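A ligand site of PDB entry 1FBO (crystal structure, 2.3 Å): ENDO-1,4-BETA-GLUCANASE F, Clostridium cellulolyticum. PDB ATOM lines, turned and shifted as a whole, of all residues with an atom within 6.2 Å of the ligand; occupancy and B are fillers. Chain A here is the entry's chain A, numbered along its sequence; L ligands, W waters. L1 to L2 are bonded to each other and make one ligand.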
ATOM      1  N   HIS A  36       1.714   4.666  14.636  1.00  0.00           N
ATOM      2  CA  HIS A  36       1.285   3.458  13.959  1.00  0.00           C
ATOM      3  C   HIS A  36       0.262   3.872  12.906  1.00  0.00           C
ATOM      4  O   HIS A  36       0.232   3.345  11.791  1.00  0.00           O
ATOM      5  CB  HIS A  36       0.620   2.494  14.947  1.00  0.00           C
ATOM      6  CG  HIS A  36       0.032   1.283  14.299  1.00  0.00           C
ATOM      7  ND1 HIS A  36       0.794   0.228  13.850  1.00  0.00           N
ATOM      8  CD2 HIS A  36      -1.253   0.984  13.972  1.00  0.00           C
ATOM      9  CE1 HIS A  36       0.007  -0.668  13.267  1.00  0.00           C
ATOM     10  NE2 HIS A  36      -1.239  -0.229  13.333  1.00  0.00           N
ATOM     11  N   VAL A  43      -6.758  -0.745  17.414  1.00  0.00           N
ATOM     12  CA  VAL A  43      -6.382  -1.975  18.112  1.00  0.00           C
ATOM     13  C   VAL A  43      -6.229  -3.156  17.138  1.00  0.00           C
ATOM     14  O   VAL A  43      -7.214  -3.601  16.555  1.00  0.00           O
ATOM     15  CB  VAL A  43      -7.419  -2.381  19.194  1.00  0.00           C
ATOM     16  CG1 VAL A  43      -6.973  -3.666  19.875  1.00  0.00           C
ATOM     17  CG2 VAL A  43      -7.591  -1.257  20.221  1.00  0.00           C
ATOM     18  N   GLU A  44      -4.998  -3.642  16.956  1.00  0.00           N
ATOM     19  CA  GLU A  44      -4.732  -4.770  16.065  1.00  0.00           C
ATOM     20  C   GLU A  44      -3.420  -5.505  16.371  1.00  0.00           C
ATOM     21  O   GLU A  44      -3.344  -6.730  16.255  1.00  0.00           O
ATOM     22  CB  GLU A  44      -4.769  -4.327  14.593  1.00  0.00           C
ATOM     23  CG  GLU A  44      -3.875  -3.148  14.251  1.00  0.00           C
ATOM     24  CD  GLU A  44      -4.111  -2.662  12.828  1.00  0.00           C
ATOM     25  OE1 GLU A  44      -5.287  -2.625  12.416  1.00  0.00           O
ATOM     26  OE2 GLU A  44      -3.129  -2.308  12.137  1.00  0.00           O
ATOM     27  N   ALA A  45      -2.379  -4.767  16.729  1.00  0.00           N
ATOM     28  CA  ALA A  45      -1.088  -5.333  17.117  1.00  0.00           C
ATOM     29  C   ALA A  45      -0.852  -4.450  18.341  1.00  0.00           C
ATOM     30  O   ALA A  45      -0.792  -4.937  19.472  1.00  0.00           O
ATOM     31  CB  ALA A  45      -0.041  -5.121  16.029  1.00  0.00           C
ATOM     32  N   PRO A  46      -0.678  -3.126  18.127  1.00  0.00           N
ATOM     33  CA  PRO A  46      -0.496  -2.293  19.323  1.00  0.00           C
ATOM     34  C   PRO A  46      -1.970  -2.030  19.689  1.00  0.00           C
ATOM     35  O   PRO A  46      -2.856  -2.329  18.892  1.00  0.00           O
ATOM     36  CB  PRO A  46       0.220  -1.060  18.775  1.00  0.00           C
ATOM     37  CG  PRO A  46      -0.319  -0.942  17.391  1.00  0.00           C
ATOM     38  CD  PRO A  46      -0.294  -2.373  16.916  1.00  0.00           C
ATOM     39  N   THR A  53       5.990   1.470  16.812  1.00  0.00           N
ATOM     40  CA  THR A  53       6.706   0.194  16.849  1.00  0.00           C
ATOM     41  C   THR A  53       8.010   0.259  16.075  1.00  0.00           C
ATOM     42  O   THR A  53       8.182   1.130  15.213  1.00  0.00           O
ATOM     43  CB  THR A  53       5.874  -0.915  16.219  1.00  0.00           C
ATOM     44  OG1 THR A  53       5.577  -0.555  14.864  1.00  0.00           O
ATOM     45  CG2 THR A  53       4.580  -1.136  16.981  1.00  0.00           C
ATOM     46  N   GLU A  55       8.732  -1.593  13.919  1.00  0.00           N
ATOM     47  CA  GLU A  55       8.291  -1.906  12.563  1.00  0.00           C
ATOM     48  C   GLU A  55       8.053  -0.607  11.794  1.00  0.00           C
ATOM     49  O   GLU A  55       8.380  -0.501  10.612  1.00  0.00           O
ATOM     50  CB  GLU A  55       6.999  -2.719  12.636  1.00  0.00           C
ATOM     51  CG  GLU A  55       6.163  -2.739  11.370  1.00  0.00           C
ATOM     52  CD  GLU A  55       4.854  -3.460  11.594  1.00  0.00           C
ATOM     53  OE1 GLU A  55       4.861  -4.711  11.741  1.00  0.00           O
ATOM     54  OE2 GLU A  55       3.801  -2.779  11.642  1.00  0.00           O
ATOM     55  N   ASP A 230      12.222  -9.112  13.024  1.00  0.00           N
ATOM     56  CA  ASP A 230      11.882  -8.799  11.650  1.00  0.00           C
ATOM     57  C   ASP A 230      12.070  -7.304  11.336  1.00  0.00           C
ATOM     58  O   ASP A 230      12.427  -6.924  10.216  1.00  0.00           O
ATOM     59  CB  ASP A 230      10.453  -9.278  11.318  1.00  0.00           C
ATOM     60  CG  ASP A 230       9.375  -8.499  12.049  1.00  0.00           C
ATOM     61  OD1 ASP A 230       9.622  -8.047  13.194  1.00  0.00           O
ATOM     62  OD2 ASP A 230       8.272  -8.355  11.477  1.00  0.00           O
ATOM     63  N   PRO A 406      -5.610 -13.861  16.940  1.00  0.00           N
ATOM     64  CA  PRO A 406      -5.839 -14.860  15.897  1.00  0.00           C
ATOM     65  C   PRO A 406      -4.548 -15.600  15.513  1.00  0.00           C
ATOM     66  O   PRO A 406      -3.460 -15.177  15.884  1.00  0.00           O
ATOM     67  CB  PRO A 406      -6.371 -14.015  14.746  1.00  0.00           C
ATOM     68  CG  PRO A 406      -5.509 -12.788  14.850  1.00  0.00           C
ATOM     69  CD  PRO A 406      -5.545 -12.508  16.355  1.00  0.00           C
ATOM     70  N   GLY A 407      -4.690 -16.692  14.765  1.00  0.00           N
ATOM     71  CA  GLY A 407      -3.514 -17.443  14.356  1.00  0.00           C
ATOM     72  C   GLY A 407      -2.528 -16.560  13.628  1.00  0.00           C
ATOM     73  O   GLY A 407      -2.893 -15.895  12.647  1.00  0.00           O
ATOM     74  N   SER A 408      -1.278 -16.539  14.098  1.00  0.00           N
ATOM     75  CA  SER A 408      -0.223 -15.712  13.501  1.00  0.00           C
ATOM     76  C   SER A 408      -0.018 -15.943  12.005  1.00  0.00           C
ATOM     77  O   SER A 408       0.570 -15.094  11.333  1.00  0.00           O
ATOM     78  CB  SER A 408       1.106 -15.940  14.217  1.00  0.00           C
ATOM     79  OG  SER A 408       1.579 -17.260  13.997  1.00  0.00           O
ATOM     80  N   THR A 410      -2.621 -16.642   9.753  1.00  0.00           N
ATOM     81  CA  THR A 410      -3.920 -16.600   9.075  1.00  0.00           C
ATOM     82  C   THR A 410      -4.042 -15.246   8.347  1.00  0.00           C
ATOM     83  O   THR A 410      -4.983 -15.018   7.592  1.00  0.00           O
ATOM     84  CB  THR A 410      -5.121 -16.757  10.060  1.00  0.00           C
ATOM     85  OG1 THR A 410      -5.091 -15.707  11.038  1.00  0.00           O
ATOM     86  CG2 THR A 410      -5.070 -18.112  10.761  1.00  0.00           C
ATOM     87  N   TRP A 411      -3.094 -14.345   8.602  1.00  0.00           N
ATOM     88  CA  TRP A 411      -3.065 -13.023   7.971  1.00  0.00           C
ATOM     89  C   TRP A 411      -2.213 -13.114   6.698  1.00  0.00           C
ATOM     90  O   TRP A 411      -1.036 -13.467   6.758  1.00  0.00           O
ATOM     91  CB  TRP A 411      -2.427 -11.998   8.922  1.00  0.00           C
ATOM     92  CG  TRP A 411      -2.328 -10.597   8.356  1.00  0.00           C
ATOM     93  CD1 TRP A 411      -3.351  -9.841   7.862  1.00  0.00           C
ATOM     94  CD2 TRP A 411      -1.139  -9.785   8.260  1.00  0.00           C
ATOM     95  NE1 TRP A 411      -2.876  -8.611   7.464  1.00  0.00           N
ATOM     96  CE2 TRP A 411      -1.522  -8.545   7.689  1.00  0.00           C
ATOM     97  CE3 TRP A 411       0.205  -9.987   8.588  1.00  0.00           C
ATOM     98  CZ2 TRP A 411      -0.614  -7.509   7.457  1.00  0.00           C
ATOM     99  CZ3 TRP A 411       1.122  -8.960   8.349  1.00  0.00           C
ATOM    100  CH2 TRP A 411       0.704  -7.733   7.782  1.00  0.00           C
ATOM    101  N   MET A 414       1.768 -11.772   6.016  1.00  0.00           N
ATOM    102  CA  MET A 414       3.042 -12.448   6.236  1.00  0.00           C
ATOM    103  C   MET A 414       3.586 -13.024   4.920  1.00  0.00           C
ATOM    104  O   MET A 414       4.784 -13.142   4.741  1.00  0.00           O
ATOM    105  CB  MET A 414       2.892 -13.570   7.276  1.00  0.00           C
ATOM    106  CG  MET A 414       2.599 -13.075   8.689  1.00  0.00           C
ATOM    107  SD  MET A 414       3.965 -12.117   9.402  1.00  0.00           S
ATOM    108  CE  MET A 414       3.441 -11.971  11.081  1.00  0.00           C
ATOM    109  N   TRP A 417       5.146  -9.747   2.899  1.00  0.00           N
ATOM    110  CA  TRP A 417       6.249  -9.129   3.634  1.00  0.00           C
ATOM    111  C   TRP A 417       7.519  -9.977   3.549  1.00  0.00           C
ATOM    112  O   TRP A 417       8.605  -9.478   3.262  1.00  0.00           O
ATOM    113  CB  TRP A 417       5.888  -8.942   5.101  1.00  0.00           C
ATOM    114  CG  TRP A 417       5.154  -7.681   5.403  1.00  0.00           C
ATOM    115  CD1 TRP A 417       4.696  -6.761   4.509  1.00  0.00           C
ATOM    116  CD2 TRP A 417       4.791  -7.205   6.710  1.00  0.00           C
ATOM    117  NE1 TRP A 417       4.066  -5.734   5.174  1.00  0.00           N
ATOM    118  CE2 TRP A 417       4.114  -5.981   6.526  1.00  0.00           C
ATOM    119  CE3 TRP A 417       4.984  -7.694   8.008  1.00  0.00           C
ATOM    120  CZ2 TRP A 417       3.614  -5.241   7.596  1.00  0.00           C
ATOM    121  CZ3 TRP A 417       4.486  -6.946   9.072  1.00  0.00           C
ATOM    122  CH2 TRP A 417       3.807  -5.736   8.859  1.00  0.00           C
ATOM    123  N   ASP A 494      -6.872  -4.772   1.465  1.00  0.00           N
ATOM    124  CA  ASP A 494      -5.904  -4.211   2.406  1.00  0.00           C
ATOM    125  C   ASP A 494      -4.812  -3.541   1.565  1.00  0.00           C
ATOM    126  O   ASP A 494      -3.977  -4.224   0.952  1.00  0.00           O
ATOM    127  CB  ASP A 494      -5.310  -5.321   3.284  1.00  0.00           C
ATOM    128  CG  ASP A 494      -4.358  -4.784   4.343  1.00  0.00           C
ATOM    129  OD1 ASP A 494      -3.386  -4.080   3.976  1.00  0.00           O
ATOM    130  OD2 ASP A 494      -4.572  -5.083   5.529  1.00  0.00           O
ATOM    131  N   GLY A 496      -2.112  -2.063   2.362  1.00  0.00           N
ATOM    132  CA  GLY A 496      -0.736  -2.285   2.756  1.00  0.00           C
ATOM    133  C   GLY A 496      -0.229  -3.585   2.163  1.00  0.00           C
ATOM    134  O   GLY A 496       0.874  -3.661   1.602  1.00  0.00           O
ATOM    135  N   CYS A 497      -1.040  -4.634   2.297  1.00  0.00           N
ATOM    136  CA  CYS A 497      -0.694  -5.937   1.761  1.00  0.00           C
ATOM    137  C   CYS A 497      -0.626  -5.887   0.228  1.00  0.00           C
ATOM    138  O   CYS A 497       0.235  -6.511  -0.374  1.00  0.00           O
ATOM    139  CB  CYS A 497      -1.715  -6.985   2.211  1.00  0.00           C
ATOM    140  SG  CYS A 497      -1.780  -7.214   4.008  1.00  0.00           S
ATOM    141  N   GLU A 542     -12.903  -0.206   5.884  1.00  0.00           N
ATOM    142  CA  GLU A 542     -12.736  -1.609   6.246  1.00  0.00           C
ATOM    143  C   GLU A 542     -13.525  -1.889   7.524  1.00  0.00           C
ATOM    144  O   GLU A 542     -13.771  -0.981   8.324  1.00  0.00           O
ATOM    145  CB  GLU A 542     -11.253  -1.945   6.453  1.00  0.00           C
ATOM    146  CG  GLU A 542     -10.646  -1.430   7.738  1.00  0.00           C
ATOM    147  CD  GLU A 542      -9.161  -1.746   7.847  1.00  0.00           C
ATOM    148  OE1 GLU A 542      -8.349  -1.068   7.167  1.00  0.00           O
ATOM    149  OE2 GLU A 542      -8.798  -2.669   8.612  1.00  0.00           O
ATOM    150  N   ARG A 544     -14.101  -3.590  11.241  1.00  0.00           N
ATOM    151  CA  ARG A 544     -13.310  -3.942  12.426  1.00  0.00           C
ATOM    152  C   ARG A 544     -14.131  -4.962  13.220  1.00  0.00           C
ATOM    153  O   ARG A 544     -14.761  -4.630  14.229  1.00  0.00           O
ATOM    154  CB  ARG A 544     -13.047  -2.690  13.253  1.00  0.00           C
ATOM    155  CG  ARG A 544     -12.619  -1.487  12.417  1.00  0.00           C
ATOM    156  CD  ARG A 544     -11.294  -1.740  11.719  1.00  0.00           C
ATOM    157  NE  ARG A 544     -10.170  -1.564  12.625  1.00  0.00           N
ATOM    158  CZ  ARG A 544      -9.015  -2.226  12.544  1.00  0.00           C
ATOM    159  NH1 ARG A 544      -8.829  -3.131  11.590  1.00  0.00           N
ATOM    160  NH2 ARG A 544      -8.055  -1.975  13.423  1.00  0.00           N
ATOM    161  N   ARG A 609      -2.604   3.717   8.152  1.00  0.00           N
ATOM    162  CA  ARG A 609      -1.490   3.085   8.857  1.00  0.00           C
ATOM    163  C   ARG A 609      -0.177   3.521   8.226  1.00  0.00           C
ATOM    164  O   ARG A 609       0.026   3.362   7.016  1.00  0.00           O
ATOM    165  CB  ARG A 609      -1.613   1.567   8.778  1.00  0.00           C
ATOM    166  CG  ARG A 609      -2.910   0.984   9.334  1.00  0.00           C
ATOM    167  CD  ARG A 609      -2.888  -0.543   9.238  1.00  0.00           C
ATOM    168  NE  ARG A 609      -4.076  -1.185   9.802  1.00  0.00           N
ATOM    169  CZ  ARG A 609      -5.257  -1.253   9.201  1.00  0.00           C
ATOM    170  NH1 ARG A 609      -5.433  -0.722   7.984  1.00  0.00           N
ATOM    171  NH2 ARG A 609      -6.270  -1.857   9.796  1.00  0.00           N
ATOM    172  N   TRP A 611       2.890   2.281   8.117  1.00  0.00           N
ATOM    173  CA  TRP A 611       3.606   1.304   7.313  1.00  0.00           C
ATOM    174  C   TRP A 611       2.919   1.050   5.973  1.00  0.00           C
ATOM    175  O   TRP A 611       3.597   0.852   4.959  1.00  0.00           O
ATOM    176  CB  TRP A 611       3.784  -0.029   8.054  1.00  0.00           C
ATOM    177  CG  TRP A 611       2.552  -0.863   8.217  1.00  0.00           C
ATOM    178  CD1 TRP A 611       1.742  -0.935   9.316  1.00  0.00           C
ATOM    179  CD2 TRP A 611       2.027  -1.816   7.278  1.00  0.00           C
ATOM    180  NE1 TRP A 611       0.757  -1.874   9.127  1.00  0.00           N
ATOM    181  CE2 TRP A 611       0.916  -2.431   7.885  1.00  0.00           C
ATOM    182  CE3 TRP A 611       2.401  -2.209   5.989  1.00  0.00           C
ATOM    183  CZ2 TRP A 611       0.158  -3.426   7.237  1.00  0.00           C
ATOM    184  CZ3 TRP A 611       1.653  -3.207   5.342  1.00  0.00           C
ATOM    185  CH2 TRP A 611       0.547  -3.795   5.979  1.00  0.00           C
HETATM  186  C1  LIG L   1      -4.339  -9.880  11.689  1.00  0.00           C
HETATM  187  C2  LIG L   1      -3.508  -8.614  11.536  1.00  0.00           C
HETATM  188  C3  LIG L   1      -4.363  -7.436  11.058  1.00  0.00           C
HETATM  189  C4  LIG L   1      -3.558  -6.397  10.277  1.00  0.00           C
HETATM  190  C5  LIG L   1      -4.531  -5.432   9.617  1.00  0.00           C
HETATM  191  C6  LIG L   1      -3.837  -4.409   8.733  1.00  0.00           C
HETATM  192  O1  LIG L   1      -3.551 -10.966  12.151  1.00  0.00           O
HETATM  193  O2  LIG L   1      -2.915  -8.307  12.791  1.00  0.00           O
HETATM  194  O3  LIG L   1      -4.964  -6.818  12.186  1.00  0.00           O
HETATM  195  O4  LIG L   1      -2.692  -5.658  11.159  1.00  0.00           O
HETATM  196  O5  LIG L   1      -5.486  -6.161   8.848  1.00  0.00           O
HETATM  197  O6  LIG L   1      -2.993  -5.038   7.789  1.00  0.00           O
HETATM  198  C1  LG2 L   2      -1.327  -5.740  10.975  1.00  0.00           C
HETATM  199  C2  LG2 L   2      -0.653  -4.541  11.672  1.00  0.00           C
HETATM  200  C3  LG2 L   2       0.876  -4.681  11.713  1.00  0.00           C
HETATM  201  C4  LG2 L   2       1.244  -6.049  12.292  1.00  0.00           C
HETATM  202  C5  LG2 L   2       0.558  -7.134  11.470  1.00  0.00           C
HETATM  203  C6  LG2 L   2       0.882  -8.537  11.965  1.00  0.00           C
HETATM  204  O1  LG2 L   2      -0.996  -3.335  10.990  1.00  0.00           O
HETATM  205  O2  LG2 L   2       1.435  -3.647  12.509  1.00  0.00           O
HETATM  206  O3  LG2 L   2       2.655  -6.225  12.250  1.00  0.00           O
HETATM  207  O4  LG2 L   2      -0.871  -6.977  11.544  1.00  0.00           O
HETATM  208  O5  LG2 L   2       0.593  -8.673  13.356  1.00  0.00           O
HETATM  209  O   HOH W   1      -5.745 -12.726  10.926  1.00  0.00           O
HETATM  210  O   HOH W   2      -5.235  -7.354   6.391  1.00  0.00           O
HETATM  211  O   HOH W   3       2.646 -10.195  14.741  1.00  0.00           O
HETATM  212  O   HOH W   4       4.468  -6.938  14.830  1.00  0.00           O
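The backbone NH of Glu 55 sits close to the side-chain hydroxyl of Thr 53. The side-chain carboxylate (OE2) of Glu 44 lies within salt-bridge range of the guanidinium group (NE) of Arg 609, 2.8 Å away. The side-chain carboxylate (OE1) of Glu 44 is in salt-bridge range of the guanidinium group (NH2) of Arg 544, 3.0 Å away. The side-chain carboxylate (OD1) of Asp 494 lies within hydrogen-bond range of the backbone NH (N) of Gly 496 (2.9 Å). The backbone NH (N) of Cys 497 sits at hydrogen-bond distance from the side-chain carboxylate (OD1) of Asp 494 (2.9 Å). OE2 of Glu 44 sits at hydrogen-bond distance from NE2 of His 36, 3.1 Å away. OE2 of Glu 542 is in salt-bridge range of NH2 of Arg 609 (2.9 Å).
His 36 touches the ligand. CG of Pro 406 touches O1 of LIG L1 (3.8 Å). Trp 411 touches the ligand. Trp 417 touches the ligand. NE of Arg 609 touches C6 of LIG L1, 3.4 Å away. Hydrophobic or aromatic side chains that line the ligand: His 36, Pro 406, Trp 411, Trp 417 and Trp 611.
Water W2 lies within hydrogen-bond range of the side-chain carboxylate of Asp 494, an oxygen (O5) of LIG L1 and the indole nitrogen of Trp 411. Water W1 bridges the side-chain hydroxyl (OG1) of Thr 410 (3.1 Å) and an oxygen (O1) of LIG L1 (3.1 Å).
The side-chain carboxylate of Glu 44 sits at hydrogen-bond distance from an oxygen (O1) of LG2 L2 (2.6 Å). An oxygen (O1) of LG2 L2 sits at hydrogen-bond distance from the indole nitrogen (NE1) of Trp 611, 2.9 Å away. An oxygen (O6) of LIG L1 is in hydrogen-bond range of the side-chain carboxylate of Asp 494 (2.8 Å). The side-chain carboxylate of Glu 55 sits at hydrogen-bond distance from an oxygen (O2) of LG2 L2, at 2.7 Å.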
